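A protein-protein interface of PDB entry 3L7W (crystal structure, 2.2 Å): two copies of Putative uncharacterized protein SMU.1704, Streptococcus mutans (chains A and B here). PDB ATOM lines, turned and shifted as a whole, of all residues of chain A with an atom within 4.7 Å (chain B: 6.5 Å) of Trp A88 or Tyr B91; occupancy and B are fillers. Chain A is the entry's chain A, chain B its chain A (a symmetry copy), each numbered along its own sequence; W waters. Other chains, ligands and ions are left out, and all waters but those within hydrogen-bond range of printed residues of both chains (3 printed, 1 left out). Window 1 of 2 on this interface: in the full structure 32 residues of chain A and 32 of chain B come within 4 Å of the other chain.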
ATOM      1  N   TYR A   3     -27.085  13.503 -32.890  1.00  0.00           N
ATOM      2  CA  TYR A   3     -27.748  13.433 -31.605  1.00  0.00           C
ATOM      3  C   TYR A   3     -28.252  14.803 -31.213  1.00  0.00           C
ATOM      4  O   TYR A   3     -27.592  15.811 -31.468  1.00  0.00           O
ATOM      5  CB  TYR A   3     -26.796  12.891 -30.567  1.00  0.00           C
ATOM      6  CG  TYR A   3     -26.330  11.478 -30.838  1.00  0.00           C
ATOM      7  CD1 TYR A   3     -27.211  10.410 -30.732  1.00  0.00           C
ATOM      8  CD2 TYR A   3     -25.007  11.207 -31.175  1.00  0.00           C
ATOM      9  CE1 TYR A   3     -26.792   9.116 -30.947  1.00  0.00           C
ATOM     10  CE2 TYR A   3     -24.577   9.905 -31.406  1.00  0.00           C
ATOM     11  CZ  TYR A   3     -25.484   8.864 -31.289  1.00  0.00           C
ATOM     12  OH  TYR A   3     -25.098   7.559 -31.506  1.00  0.00           O
ATOM     13  N   PRO A   4     -29.439  14.847 -30.597  1.00  0.00           N
ATOM     14  CA  PRO A   4     -29.986  16.121 -30.139  1.00  0.00           C
ATOM     15  C   PRO A   4     -29.231  16.597 -28.908  1.00  0.00           C
ATOM     16  O   PRO A   4     -28.564  15.798 -28.259  1.00  0.00           O
ATOM     17  CB  PRO A   4     -31.422  15.775 -29.731  1.00  0.00           C
ATOM     18  CG  PRO A   4     -31.516  14.268 -29.737  1.00  0.00           C
ATOM     19  CD  PRO A   4     -30.174  13.697 -30.057  1.00  0.00           C
ATOM     20  N   VAL A   5     -29.356  17.884 -28.601  1.00  0.00           N
ATOM     21  CA  VAL A   5     -28.774  18.461 -27.408  1.00  0.00           C
ATOM     22  C   VAL A   5     -29.916  18.914 -26.495  1.00  0.00           C
ATOM     23  O   VAL A   5     -30.680  19.799 -26.843  1.00  0.00           O
ATOM     24  CB  VAL A   5     -27.928  19.683 -27.770  1.00  0.00           C
ATOM     25  CG1 VAL A   5     -27.424  20.404 -26.496  1.00  0.00           C
ATOM     26  CG2 VAL A   5     -26.798  19.288 -28.701  1.00  0.00           C
ATOM     27  N   SER A   6     -30.020  18.318 -25.319  1.00  0.00           N
ATOM     28  CA  SER A   6     -31.101  18.658 -24.413  1.00  0.00           C
ATOM     29  C   SER A   6     -30.935  20.082 -23.896  1.00  0.00           C
ATOM     30  O   SER A   6     -29.838  20.635 -23.930  1.00  0.00           O
ATOM     31  CB  SER A   6     -31.131  17.677 -23.244  1.00  0.00           C
ATOM     32  OG  SER A   6     -29.981  17.831 -22.425  1.00  0.00           O
ATOM     33  N   LEU A   9     -28.268  20.403 -21.478  1.00  0.00           N
ATOM     34  CA  LEU A   9     -26.935  20.413 -22.070  1.00  0.00           C
ATOM     35  C   LEU A   9     -26.654  21.794 -22.663  1.00  0.00           C
ATOM     36  O   LEU A   9     -25.529  22.274 -22.621  1.00  0.00           O
ATOM     37  CB  LEU A   9     -26.823  19.335 -23.144  1.00  0.00           C
ATOM     38  CG  LEU A   9     -25.653  18.373 -23.024  1.00  0.00           C
ATOM     39  CD1 LEU A   9     -25.574  17.462 -24.261  1.00  0.00           C
ATOM     40  CD2 LEU A   9     -24.359  19.128 -22.818  1.00  0.00           C
ATOM     41  N   TYR A  12     -25.434  23.915 -19.914  1.00  0.00           N
ATOM     42  CA  TYR A  12     -24.028  23.581 -19.780  1.00  0.00           C
ATOM     43  C   TYR A  12     -23.222  24.362 -20.807  1.00  0.00           C
ATOM     44  O   TYR A  12     -22.286  25.073 -20.465  1.00  0.00           O
ATOM     45  CB  TYR A  12     -23.831  22.071 -19.949  1.00  0.00           C
ATOM     46  CG  TYR A  12     -22.405  21.599 -19.875  1.00  0.00           C
ATOM     47  CD1 TYR A  12     -21.535  22.100 -18.925  1.00  0.00           C
ATOM     48  CD2 TYR A  12     -21.936  20.628 -20.749  1.00  0.00           C
ATOM     49  CE1 TYR A  12     -20.239  21.664 -18.857  1.00  0.00           C
ATOM     50  CE2 TYR A  12     -20.644  20.183 -20.693  1.00  0.00           C
ATOM     51  CZ  TYR A  12     -19.798  20.703 -19.743  1.00  0.00           C
ATOM     52  OH  TYR A  12     -18.509  20.261 -19.673  1.00  0.00           O
ATOM     53  N   ILE A  35     -23.436  22.633 -32.607  1.00  0.00           N
ATOM     54  CA  ILE A  35     -23.753  21.271 -32.216  1.00  0.00           C
ATOM     55  C   ILE A  35     -25.246  21.065 -32.046  1.00  0.00           C
ATOM     56  O   ILE A  35     -25.722  19.937 -32.080  1.00  0.00           O
ATOM     57  CB  ILE A  35     -23.003  20.815 -30.932  1.00  0.00           C
ATOM     58  CG1 ILE A  35     -23.365  19.364 -30.621  1.00  0.00           C
ATOM     59  CG2 ILE A  35     -23.321  21.732 -29.727  1.00  0.00           C
ATOM     60  CD1 ILE A  35     -22.271  18.580 -29.965  1.00  0.00           C
ATOM     61  N   LEU A  84     -22.190  20.902 -13.695  1.00  0.00           N
ATOM     62  CA  LEU A  84     -22.616  20.498 -15.049  1.00  0.00           C
ATOM     63  C   LEU A  84     -21.500  19.816 -15.819  1.00  0.00           C
ATOM     64  O   LEU A  84     -21.737  18.849 -16.522  1.00  0.00           O
ATOM     65  CB  LEU A  84     -23.104  21.696 -15.859  1.00  0.00           C
ATOM     66  CG  LEU A  84     -24.322  22.420 -15.291  1.00  0.00           C
ATOM     67  CD1 LEU A  84     -24.634  23.653 -16.129  1.00  0.00           C
ATOM     68  CD2 LEU A  84     -25.497  21.469 -15.237  1.00  0.00           C
ATOM     69  N   THR A  85     -20.281  20.323 -15.682  1.00  0.00           N
ATOM     70  CA  THR A  85     -19.137  19.699 -16.320  1.00  0.00           C
ATOM     71  C   THR A  85     -18.965  18.294 -15.772  1.00  0.00           C
ATOM     72  O   THR A  85     -18.830  17.334 -16.524  1.00  0.00           O
ATOM     73  CB  THR A  85     -17.864  20.496 -16.058  1.00  0.00           C
ATOM     74  OG1 THR A  85     -18.036  21.808 -16.590  1.00  0.00           O
ATOM     75  CG2 THR A  85     -16.675  19.835 -16.737  1.00  0.00           C
ATOM     76  N   LYS A  86     -18.984  18.193 -14.450  1.00  0.00           N
ATOM     77  CA  LYS A  86     -18.868  16.931 -13.748  1.00  0.00           C
ATOM     78  C   LYS A  86     -19.945  15.940 -14.215  1.00  0.00           C
ATOM     79  O   LYS A  86     -19.643  14.796 -14.557  1.00  0.00           O
ATOM     80  CB  LYS A  86     -18.996  17.168 -12.243  1.00  0.00           C
ATOM     81  CG  LYS A  86     -18.973  15.903 -11.403  1.00  0.00           C
ATOM     82  CD  LYS A  86     -19.500  16.166  -9.998  1.00  0.00           C
ATOM     83  CE  LYS A  86     -18.671  17.211  -9.285  1.00  0.00           C
ATOM     84  NZ  LYS A  86     -19.047  17.271  -7.849  1.00  0.00           N
ATOM     85  N   GLU A  87     -21.195  16.386 -14.223  1.00  0.00           N
ATOM     86  CA  GLU A  87     -22.298  15.547 -14.646  1.00  0.00           C
ATOM     87  C   GLU A  87     -22.152  15.155 -16.111  1.00  0.00           C
ATOM     88  O   GLU A  87     -22.561  14.070 -16.525  1.00  0.00           O
ATOM     89  CB  GLU A  87     -23.628  16.266 -14.415  1.00  0.00           C
ATOM     90  CG  GLU A  87     -24.141  16.086 -12.996  1.00  0.00           C
ATOM     91  CD  GLU A  87     -24.090  14.633 -12.541  1.00  0.00           C
ATOM     92  OE1 GLU A  87     -24.772  13.773 -13.158  1.00  0.00           O
ATOM     93  OE2 GLU A  87     -23.367  14.348 -11.565  1.00  0.00           O
ATOM     94  N   TRP A  88     -21.571  16.050 -16.897  1.00  0.00           N
ATOM     95  CA  TRP A  88     -21.339  15.761 -18.297  1.00  0.00           C
ATOM     96  C   TRP A  88     -20.293  14.674 -18.403  1.00  0.00           C
ATOM     97  O   TRP A  88     -20.413  13.755 -19.218  1.00  0.00           O
ATOM     98  CB  TRP A  88     -20.892  17.016 -19.031  1.00  0.00           C
ATOM     99  CG  TRP A  88     -20.394  16.759 -20.405  1.00  0.00           C
ATOM    100  CD1 TRP A  88     -19.140  17.016 -20.886  1.00  0.00           C
ATOM    101  CD2 TRP A  88     -21.138  16.196 -21.498  1.00  0.00           C
ATOM    102  NE1 TRP A  88     -19.062  16.652 -22.206  1.00  0.00           N
ATOM    103  CE2 TRP A  88     -20.268  16.139 -22.604  1.00  0.00           C
ATOM    104  CE3 TRP A  88     -22.448  15.723 -21.638  1.00  0.00           C
ATOM    105  CZ2 TRP A  88     -20.669  15.636 -23.847  1.00  0.00           C
ATOM    106  CZ3 TRP A  88     -22.850  15.216 -22.885  1.00  0.00           C
ATOM    107  CH2 TRP A  88     -21.958  15.179 -23.967  1.00  0.00           C
ATOM    108  N   SER A  89     -19.269  14.770 -17.561  1.00  0.00           N
ATOM    109  CA  SER A  89     -18.198  13.785 -17.572  1.00  0.00           C
ATOM    110  C   SER A  89     -18.799  12.421 -17.256  1.00  0.00           C
ATOM    111  O   SER A  89     -18.584  11.460 -17.986  1.00  0.00           O
ATOM    112  CB  SER A  89     -17.125  14.142 -16.554  1.00  0.00           C
ATOM    113  OG  SER A  89     -16.036  13.242 -16.620  1.00  0.00           O
ATOM    114  N   VAL A  90     -19.571  12.362 -16.175  1.00  0.00           N
ATOM    115  CA  VAL A  90     -20.264  11.146 -15.773  1.00  0.00           C
ATOM    116  C   VAL A  90     -21.156  10.597 -16.890  1.00  0.00           C
ATOM    117  O   VAL A  90     -21.125   9.415 -17.191  1.00  0.00           O
ATOM    118  CB  VAL A  90     -21.116  11.401 -14.513  1.00  0.00           C
ATOM    119  CG1 VAL A  90     -22.112  10.273 -14.305  1.00  0.00           C
ATOM    120  CG2 VAL A  90     -20.216  11.543 -13.298  1.00  0.00           C
ATOM    121  N   TYR A  91     -21.955  11.468 -17.491  1.00  0.00           N
ATOM    122  CA  TYR A  91     -22.824  11.086 -18.591  1.00  0.00           C
ATOM    123  C   TYR A  91     -21.987  10.393 -19.651  1.00  0.00           C
ATOM    124  O   TYR A  91     -22.298   9.288 -20.071  1.00  0.00           O
ATOM    125  CB  TYR A  91     -23.414  12.335 -19.199  1.00  0.00           C
ATOM    126  CG  TYR A  91     -24.527  12.168 -20.208  1.00  0.00           C
ATOM    127  CD1 TYR A  91     -25.847  12.006 -19.802  1.00  0.00           C
ATOM    128  CD2 TYR A  91     -24.275  12.269 -21.564  1.00  0.00           C
ATOM    129  CE1 TYR A  91     -26.878  11.905 -20.726  1.00  0.00           C
ATOM    130  CE2 TYR A  91     -25.298  12.173 -22.494  1.00  0.00           C
ATOM    131  CZ  TYR A  91     -26.597  11.998 -22.070  1.00  0.00           C
ATOM    132  OH  TYR A  91     -27.609  11.926 -23.001  1.00  0.00           O
ATOM    133  N   LYS A  92     -20.923  11.063 -20.072  1.00  0.00           N
ATOM    134  CA  LYS A  92     -20.056  10.539 -21.105  1.00  0.00           C
ATOM    135  C   LYS A  92     -19.484   9.193 -20.721  1.00  0.00           C
ATOM    136  O   LYS A  92     -19.585   8.251 -21.495  1.00  0.00           O
ATOM    137  CB  LYS A  92     -18.908  11.501 -21.389  1.00  0.00           C
ATOM    138  CG  LYS A  92     -19.245  12.599 -22.368  1.00  0.00           C
ATOM    139  CD  LYS A  92     -17.986  13.356 -22.755  1.00  0.00           C
ATOM    140  CE  LYS A  92     -17.211  13.767 -21.511  1.00  0.00           C
ATOM    141  NZ  LYS A  92     -16.108  14.733 -21.784  1.00  0.00           N
ATOM    142  N   TYR B   2     -28.420  13.293 -14.348  1.00  0.00           N
ATOM    143  CA  TYR B   2     -28.680  14.709 -14.624  1.00  0.00           C
ATOM    144  C   TYR B   2     -29.156  14.969 -16.053  1.00  0.00           C
ATOM    145  O   TYR B   2     -30.315  15.318 -16.289  1.00  0.00           O
ATOM    146  CB  TYR B   2     -27.450  15.574 -14.359  1.00  0.00           C
ATOM    147  CG  TYR B   2     -27.799  17.051 -14.491  1.00  0.00           C
ATOM    148  CD1 TYR B   2     -28.613  17.675 -13.555  1.00  0.00           C
ATOM    149  CD2 TYR B   2     -27.357  17.800 -15.571  1.00  0.00           C
ATOM    150  CE1 TYR B   2     -28.958  19.007 -13.680  1.00  0.00           C
ATOM    151  CE2 TYR B   2     -27.690  19.137 -15.700  1.00  0.00           C
ATOM    152  CZ  TYR B   2     -28.492  19.732 -14.752  1.00  0.00           C
ATOM    153  OH  TYR B   2     -28.831  21.051 -14.884  1.00  0.00           O
ATOM    154  N   TYR B   3     -28.255  14.806 -17.012  1.00  0.00           N
ATOM    155  CA  TYR B   3     -28.611  15.077 -18.388  1.00  0.00           C
ATOM    156  C   TYR B   3     -29.519  13.984 -18.907  1.00  0.00           C
ATOM    157  O   TYR B   3     -29.341  12.812 -18.577  1.00  0.00           O
ATOM    158  CB  TYR B   3     -27.363  15.185 -19.229  1.00  0.00           C
ATOM    159  CG  TYR B   3     -26.453  16.328 -18.834  1.00  0.00           C
ATOM    160  CD1 TYR B   3     -26.836  17.645 -19.054  1.00  0.00           C
ATOM    161  CD2 TYR B   3     -25.204  16.092 -18.267  1.00  0.00           C
ATOM    162  CE1 TYR B   3     -26.004  18.693 -18.726  1.00  0.00           C
ATOM    163  CE2 TYR B   3     -24.363  17.144 -17.920  1.00  0.00           C
ATOM    164  CZ  TYR B   3     -24.777  18.445 -18.156  1.00  0.00           C
ATOM    165  OH  TYR B   3     -23.972  19.516 -17.833  1.00  0.00           O
ATOM    166  N   SER B   6     -31.439  11.195 -25.132  1.00  0.00           N
ATOM    167  CA  SER B   6     -32.396  11.256 -26.221  1.00  0.00           C
ATOM    168  C   SER B   6     -32.691   9.857 -26.749  1.00  0.00           C
ATOM    169  O   SER B   6     -31.907   8.935 -26.547  1.00  0.00           O
ATOM    170  CB  SER B   6     -31.853  12.136 -27.344  1.00  0.00           C
ATOM    171  OG  SER B   6     -30.723  11.534 -27.958  1.00  0.00           O
ATOM    172  N   LEU B   9     -29.969   8.476 -28.683  1.00  0.00           N
ATOM    173  CA  LEU B   9     -28.860   7.986 -27.873  1.00  0.00           C
ATOM    174  C   LEU B   9     -29.226   6.621 -27.288  1.00  0.00           C
ATOM    175  O   LEU B   9     -28.374   5.753 -27.152  1.00  0.00           O
ATOM    176  CB  LEU B   9     -28.537   8.978 -26.760  1.00  0.00           C
ATOM    177  CG  LEU B   9     -27.089   9.424 -26.644  1.00  0.00           C
ATOM    178  CD1 LEU B   9     -26.887  10.280 -25.382  1.00  0.00           C
ATOM    179  CD2 LEU B   9     -26.159   8.231 -26.651  1.00  0.00           C
ATOM    180  N   LYS B  86     -19.478   6.793 -33.936  1.00  0.00           N
ATOM    181  CA  LYS B  86     -18.778   7.895 -34.565  1.00  0.00           C
ATOM    182  C   LYS B  86     -19.465   9.232 -34.256  1.00  0.00           C
ATOM    183  O   LYS B  86     -18.819  10.191 -33.829  1.00  0.00           O
ATOM    184  CB  LYS B  86     -18.726   7.673 -36.077  1.00  0.00           C
ATOM    185  CG  LYS B  86     -18.084   8.807 -36.857  1.00  0.00           C
ATOM    186  CD  LYS B  86     -18.421   8.714 -38.339  1.00  0.00           C
ATOM    187  CE  LYS B  86     -17.938   7.410 -38.935  1.00  0.00           C
ATOM    188  NZ  LYS B  86     -18.057   7.448 -40.415  1.00  0.00           N
ATOM    189  N   GLU B  87     -20.773   9.291 -34.478  1.00  0.00           N
ATOM    190  CA  GLU B  87     -21.534  10.496 -34.222  1.00  0.00           C
ATOM    191  C   GLU B  87     -21.505  10.854 -32.742  1.00  0.00           C
ATOM    192  O   GLU B  87     -21.540  12.027 -32.368  1.00  0.00           O
ATOM    193  CB  GLU B  87     -22.975  10.323 -34.702  1.00  0.00           C
ATOM    194  CG  GLU B  87     -23.132  10.634 -36.181  1.00  0.00           C
ATOM    195  CD  GLU B  87     -22.461  11.946 -36.571  1.00  0.00           C
ATOM    196  OE1 GLU B  87     -22.865  13.019 -36.052  1.00  0.00           O
ATOM    197  OE2 GLU B  87     -21.528  11.905 -37.399  1.00  0.00           O
ATOM    198  N   TRP B  88     -21.448   9.833 -31.898  1.00  0.00           N
ATOM    199  CA  TRP B  88     -21.368  10.062 -30.470  1.00  0.00           C
ATOM    200  C   TRP B  88     -20.025  10.677 -30.150  1.00  0.00           C
ATOM    201  O   TRP B  88     -19.928  11.601 -29.336  1.00  0.00           O
ATOM    202  CB  TRP B  88     -21.559   8.756 -29.714  1.00  0.00           C
ATOM    203  CG  TRP B  88     -21.245   8.853 -28.266  1.00  0.00           C
ATOM    204  CD1 TRP B  88     -20.283   8.160 -27.586  1.00  0.00           C
ATOM    205  CD2 TRP B  88     -21.898   9.691 -27.299  1.00  0.00           C
ATOM    206  NE1 TRP B  88     -20.300   8.512 -26.261  1.00  0.00           N
ATOM    207  CE2 TRP B  88     -21.273   9.453 -26.059  1.00  0.00           C
ATOM    208  CE3 TRP B  88     -22.937  10.626 -27.370  1.00  0.00           C
ATOM    209  CZ2 TRP B  88     -21.663  10.113 -24.886  1.00  0.00           C
ATOM    210  CZ3 TRP B  88     -23.326  11.288 -26.193  1.00  0.00           C
ATOM    211  CH2 TRP B  88     -22.686  11.024 -24.974  1.00  0.00           C
ATOM    212  N   SER B  89     -18.984  10.176 -30.807  1.00  0.00           N
ATOM    213  CA  SER B  89     -17.640  10.685 -30.578  1.00  0.00           C
ATOM    214  C   SER B  89     -17.620  12.163 -30.947  1.00  0.00           C
ATOM    215  O   SER B  89     -17.189  12.997 -30.159  1.00  0.00           O
ATOM    216  CB  SER B  89     -16.623   9.916 -31.409  1.00  0.00           C
ATOM    217  OG  SER B  89     -15.304  10.342 -31.126  1.00  0.00           O
ATOM    218  N   VAL B  90     -18.116  12.472 -32.142  1.00  0.00           N
ATOM    219  CA  VAL B  90     -18.220  13.844 -32.615  1.00  0.00           C
ATOM    220  C   VAL B  90     -19.018  14.727 -31.649  1.00  0.00           C
ATOM    221  O   VAL B  90     -18.596  15.819 -31.308  1.00  0.00           O
ATOM    222  CB  VAL B  90     -18.876  13.886 -34.011  1.00  0.00           C
ATOM    223  CG1 VAL B  90     -19.323  15.298 -34.348  1.00  0.00           C
ATOM    224  CG2 VAL B  90     -17.902  13.375 -35.057  1.00  0.00           C
ATOM    225  N   TYR B  91     -20.176  14.241 -31.224  1.00  0.00           N
ATOM    226  CA  TYR B  91     -21.013  14.958 -30.278  1.00  0.00           C
ATOM    227  C   TYR B  91     -20.172  15.321 -29.067  1.00  0.00           C
ATOM    228  O   TYR B  91     -20.112  16.475 -28.670  1.00  0.00           O
ATOM    229  CB  TYR B  91     -22.124  14.045 -29.822  1.00  0.00           C
ATOM    230  CG  TYR B  91     -23.247  14.651 -29.014  1.00  0.00           C
ATOM    231  CD1 TYR B  91     -24.318  15.284 -29.635  1.00  0.00           C
ATOM    232  CD2 TYR B  91     -23.289  14.509 -27.639  1.00  0.00           C
ATOM    233  CE1 TYR B  91     -25.379  15.797 -28.899  1.00  0.00           C
ATOM    234  CE2 TYR B  91     -24.343  15.014 -26.895  1.00  0.00           C
ATOM    235  CZ  TYR B  91     -25.388  15.650 -27.530  1.00  0.00           C
ATOM    236  OH  TYR B  91     -26.441  16.130 -26.786  1.00  0.00           O
ATOM    237  N   LYS B  92     -19.526  14.315 -28.492  1.00  0.00           N
ATOM    238  CA  LYS B  92     -18.717  14.508 -27.309  1.00  0.00           C
ATOM    239  C   LYS B  92     -17.624  15.527 -27.544  1.00  0.00           C
ATOM    240  O   LYS B  92     -17.495  16.463 -26.767  1.00  0.00           O
ATOM    241  CB  LYS B  92     -18.082  13.195 -26.865  1.00  0.00           C
ATOM    242  CG  LYS B  92     -18.970  12.339 -25.996  1.00  0.00           C
ATOM    243  CD  LYS B  92     -18.175  11.177 -25.424  1.00  0.00           C
ATOM    244  CE  LYS B  92     -17.411  10.463 -26.530  1.00  0.00           C
ATOM    245  NZ  LYS B  92     -16.816   9.163 -26.105  1.00  0.00           N
ATOM    246  N   MET B  93     -16.830  15.344 -28.598  1.00  0.00           N
ATOM    247  CA  MET B  93     -15.717  16.235 -28.807  1.00  0.00           C
ATOM    248  C   MET B  93     -16.213  17.648 -29.058  1.00  0.00           C
ATOM    249  O   MET B  93     -15.589  18.603 -28.641  1.00  0.00           O
ATOM    250  CB  MET B  93     -14.876  15.737 -29.968  1.00  0.00           C
ATOM    251  CG  MET B  93     -14.286  14.385 -29.700  1.00  0.00           C
ATOM    252  SD  MET B  93     -13.513  13.745 -31.335  1.00  0.00           S
ATOM    253  CE  MET B  93     -12.067  14.968 -31.464  1.00  0.00           C
ATOM    254  N   THR B  94     -17.340  17.754 -29.734  1.00  0.00           N
ATOM    255  CA  THR B  94     -17.841  19.052 -30.095  1.00  0.00           C
ATOM    256  C   THR B  94     -18.300  19.780 -28.845  1.00  0.00           C
ATOM    257  O   THR B  94     -17.968  20.936 -28.654  1.00  0.00           O
ATOM    258  CB  THR B  94     -18.936  18.926 -31.123  1.00  0.00           C
ATOM    259  OG1 THR B  94     -18.375  18.313 -32.291  1.00  0.00           O
ATOM    260  CG2 THR B  94     -19.476  20.302 -31.495  1.00  0.00           C
ATOM    261  N   ILE B  95     -19.030  19.080 -27.985  1.00  0.00           N
ATOM    262  CA  ILE B  95     -19.432  19.633 -26.711  1.00  0.00           C
ATOM    263  C   ILE B  95     -18.207  20.007 -25.879  1.00  0.00           C
ATOM    264  O   ILE B  95     -18.077  21.138 -25.416  1.00  0.00           O
ATOM    265  CB  ILE B  95     -20.338  18.660 -25.976  1.00  0.00           C
ATOM    266  CG1 ILE B  95     -21.691  18.630 -26.687  1.00  0.00           C
ATOM    267  CG2 ILE B  95     -20.512  19.074 -24.522  1.00  0.00           C
ATOM    268  CD1 ILE B  95     -22.720  17.817 -25.967  1.00  0.00           C
ATOM    269  N   ASP B  96     -17.290  19.067 -25.727  1.00  0.00           N
ATOM    270  CA  ASP B  96     -16.091  19.317 -24.941  1.00  0.00           C
ATOM    271  C   ASP B  96     -15.265  20.427 -25.569  1.00  0.00           C
ATOM    272  O   ASP B  96     -14.668  21.239 -24.871  1.00  0.00           O
ATOM    273  CB  ASP B  96     -15.263  18.041 -24.822  1.00  0.00           C
ATOM    274  CG  ASP B  96     -15.900  17.024 -23.907  1.00  0.00           C
ATOM    275  OD1 ASP B  96     -16.863  17.370 -23.190  1.00  0.00           O
ATOM    276  OD2 ASP B  96     -15.428  15.879 -23.894  1.00  0.00           O
ATOM    277  N   VAL B  99     -17.149  23.562 -24.751  1.00  0.00           N
ATOM    278  CA  VAL B  99     -16.981  23.757 -23.335  1.00  0.00           C
ATOM    279  C   VAL B  99     -15.583  24.204 -22.946  1.00  0.00           C
ATOM    280  O   VAL B  99     -15.428  25.071 -22.077  1.00  0.00           O
ATOM    281  CB  VAL B  99     -17.383  22.522 -22.560  1.00  0.00           C
ATOM    282  CG1 VAL B  99     -16.863  22.605 -21.116  1.00  0.00           C
ATOM    283  CG2 VAL B  99     -18.902  22.396 -22.593  1.00  0.00           C
HETATM  284  O   HOH W   1     -28.684  13.199 -27.741  1.00  0.00           O
HETATM  285  O   HOH W   2     -29.326  13.123 -25.215  1.00  0.00           O
HETATM  286  O   HOH W   3     -28.836  15.741 -24.940  1.00  0.00           O
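N of Trp B88 touches CE2 of Tyr A3, 3.2 Å away.
CA of Val A5 touches OH of Tyr B91 (3.4 Å).
CD1 of Leu A9 touches CD1 of Ile B95, 3.3 Å away.
CE2 of Tyr A12 touches CG2 of Ile B95 (3.99 Å).
Tyr A12 touches Val B99.
O of Tyr B91 touches CD1 of Ile A35, at 3.3 Å.
Ile A35 touches Thr B94.
Tyr B3 touches Glu A87 (CE2 to C, 3.5 Å).
Trp A88 touches Tyr B91 (CH2 to CE2, 3.8 Å).
Tyr A91 touches Tyr B3.
Of the printed residues of chain B, Trp A88 touches Tyr B3 (3.2 Å), Tyr B91 (3.8 Å), Ile B95 (3.4 Å) and Asp B96 (2.5 Å).
Tyr B91 touches six residues of chain A.
Printed residues of chain A within 4 Å of Tyr B2: Leu A84 (3.2 Å) and Glu A87 (3.4 Å).
Of the printed residues of chain B, Tyr A91 touches Tyr B3, Leu B9 and Trp B88.
Of the printed residues of chain A, Glu B87 touches Tyr A3 (3.5 Å).
Printed residues of chain B within 4 Å of Tyr A3: Leu B9, Glu B87, Trp B88 and Tyr B91.
Ser B89 touches none of the printed residues of chain A.
The nearest residue of chain A that does not touch Tyr B91 is Ser A6 (4.4 Å).
The nearest printed residue of chain B that does not touch Pro A4 is Leu B9 (5.4 Å).
Water W1 lies within hydrogen-bond range of OG of Ser B6 and O of Pro A4.
Water W3 lies within hydrogen-bond range of the backbone NH (N) of Ser A6, the side-chain hydroxyl (OH) of Tyr B91 and the backbone carbonyl oxygen (O) of Pro A4.
Water W2 bridges the backbone NH (N) of Ser B6 (2.9 Å) and the side-chain hydroxyl (OH) of Tyr A91 (3.0 Å).
Along chain B the printed residues that touch a printed residue of chain A span positions 2 to 99.
Of the 16 printed residues of chain A, 11 touch a printed residue of chain B.
Hydrophobic or aromatic side chains of chain A that line the printed part of chain B: Tyr A3, Pro A4, Val A5, Leu A9, Tyr A12, Ile A35, Leu A84, Trp A88 and Tyr A91.
Among the printed residues, 29 pairs touch across the chains.
O of Pro A4 sits at hydrogen-bond distance from OH of Tyr B91 (2.6 Å).
The backbone carbonyl oxygen of Leu A84 sits at hydrogen-bond distance from the side-chain hydroxyl of Tyr B3 (2.7 Å).
The indole nitrogen (NE1) of Trp A88 is in hydrogen-bond range of the side-chain carboxylate (OD1) of Asp B96, 2.5 Å away.
The side-chain amino group of Lys A92 is in salt-bridge range of the side-chain carboxylate of Asp B96 (2.5 Å).
The side-chain hydroxyl (OG) of Ser A6 lies within hydrogen-bond range of the backbone NH (N) of Leu A9 (3.2 Å).
The side-chain hydroxyl (OG1) of Thr A85 sits close to the side-chain hydroxyl (OH) of Tyr A12, 3.5 Å away.
OG of Ser B6 sits at hydrogen-bond distance from N of Leu B9 (3.2 Å).
The backbone carbonyl oxygen of Val B90 sits at hydrogen-bond distance from the side-chain hydroxyl of Thr B94, at 2.7 Å.
Tyr A3 touches Glu B87, and with the chains exchanged Glu A87 touches Tyr B3.
Tyr A3 touches Tyr B91, and with the chains exchanged Tyr A91 touches Tyr B3.
Leu A9 touches Tyr B91, and with the chains exchanged Tyr A91 touches Leu B9.
Lys B92 touches its own counterpart, Lys A92.
10 positions are printed for both chains.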
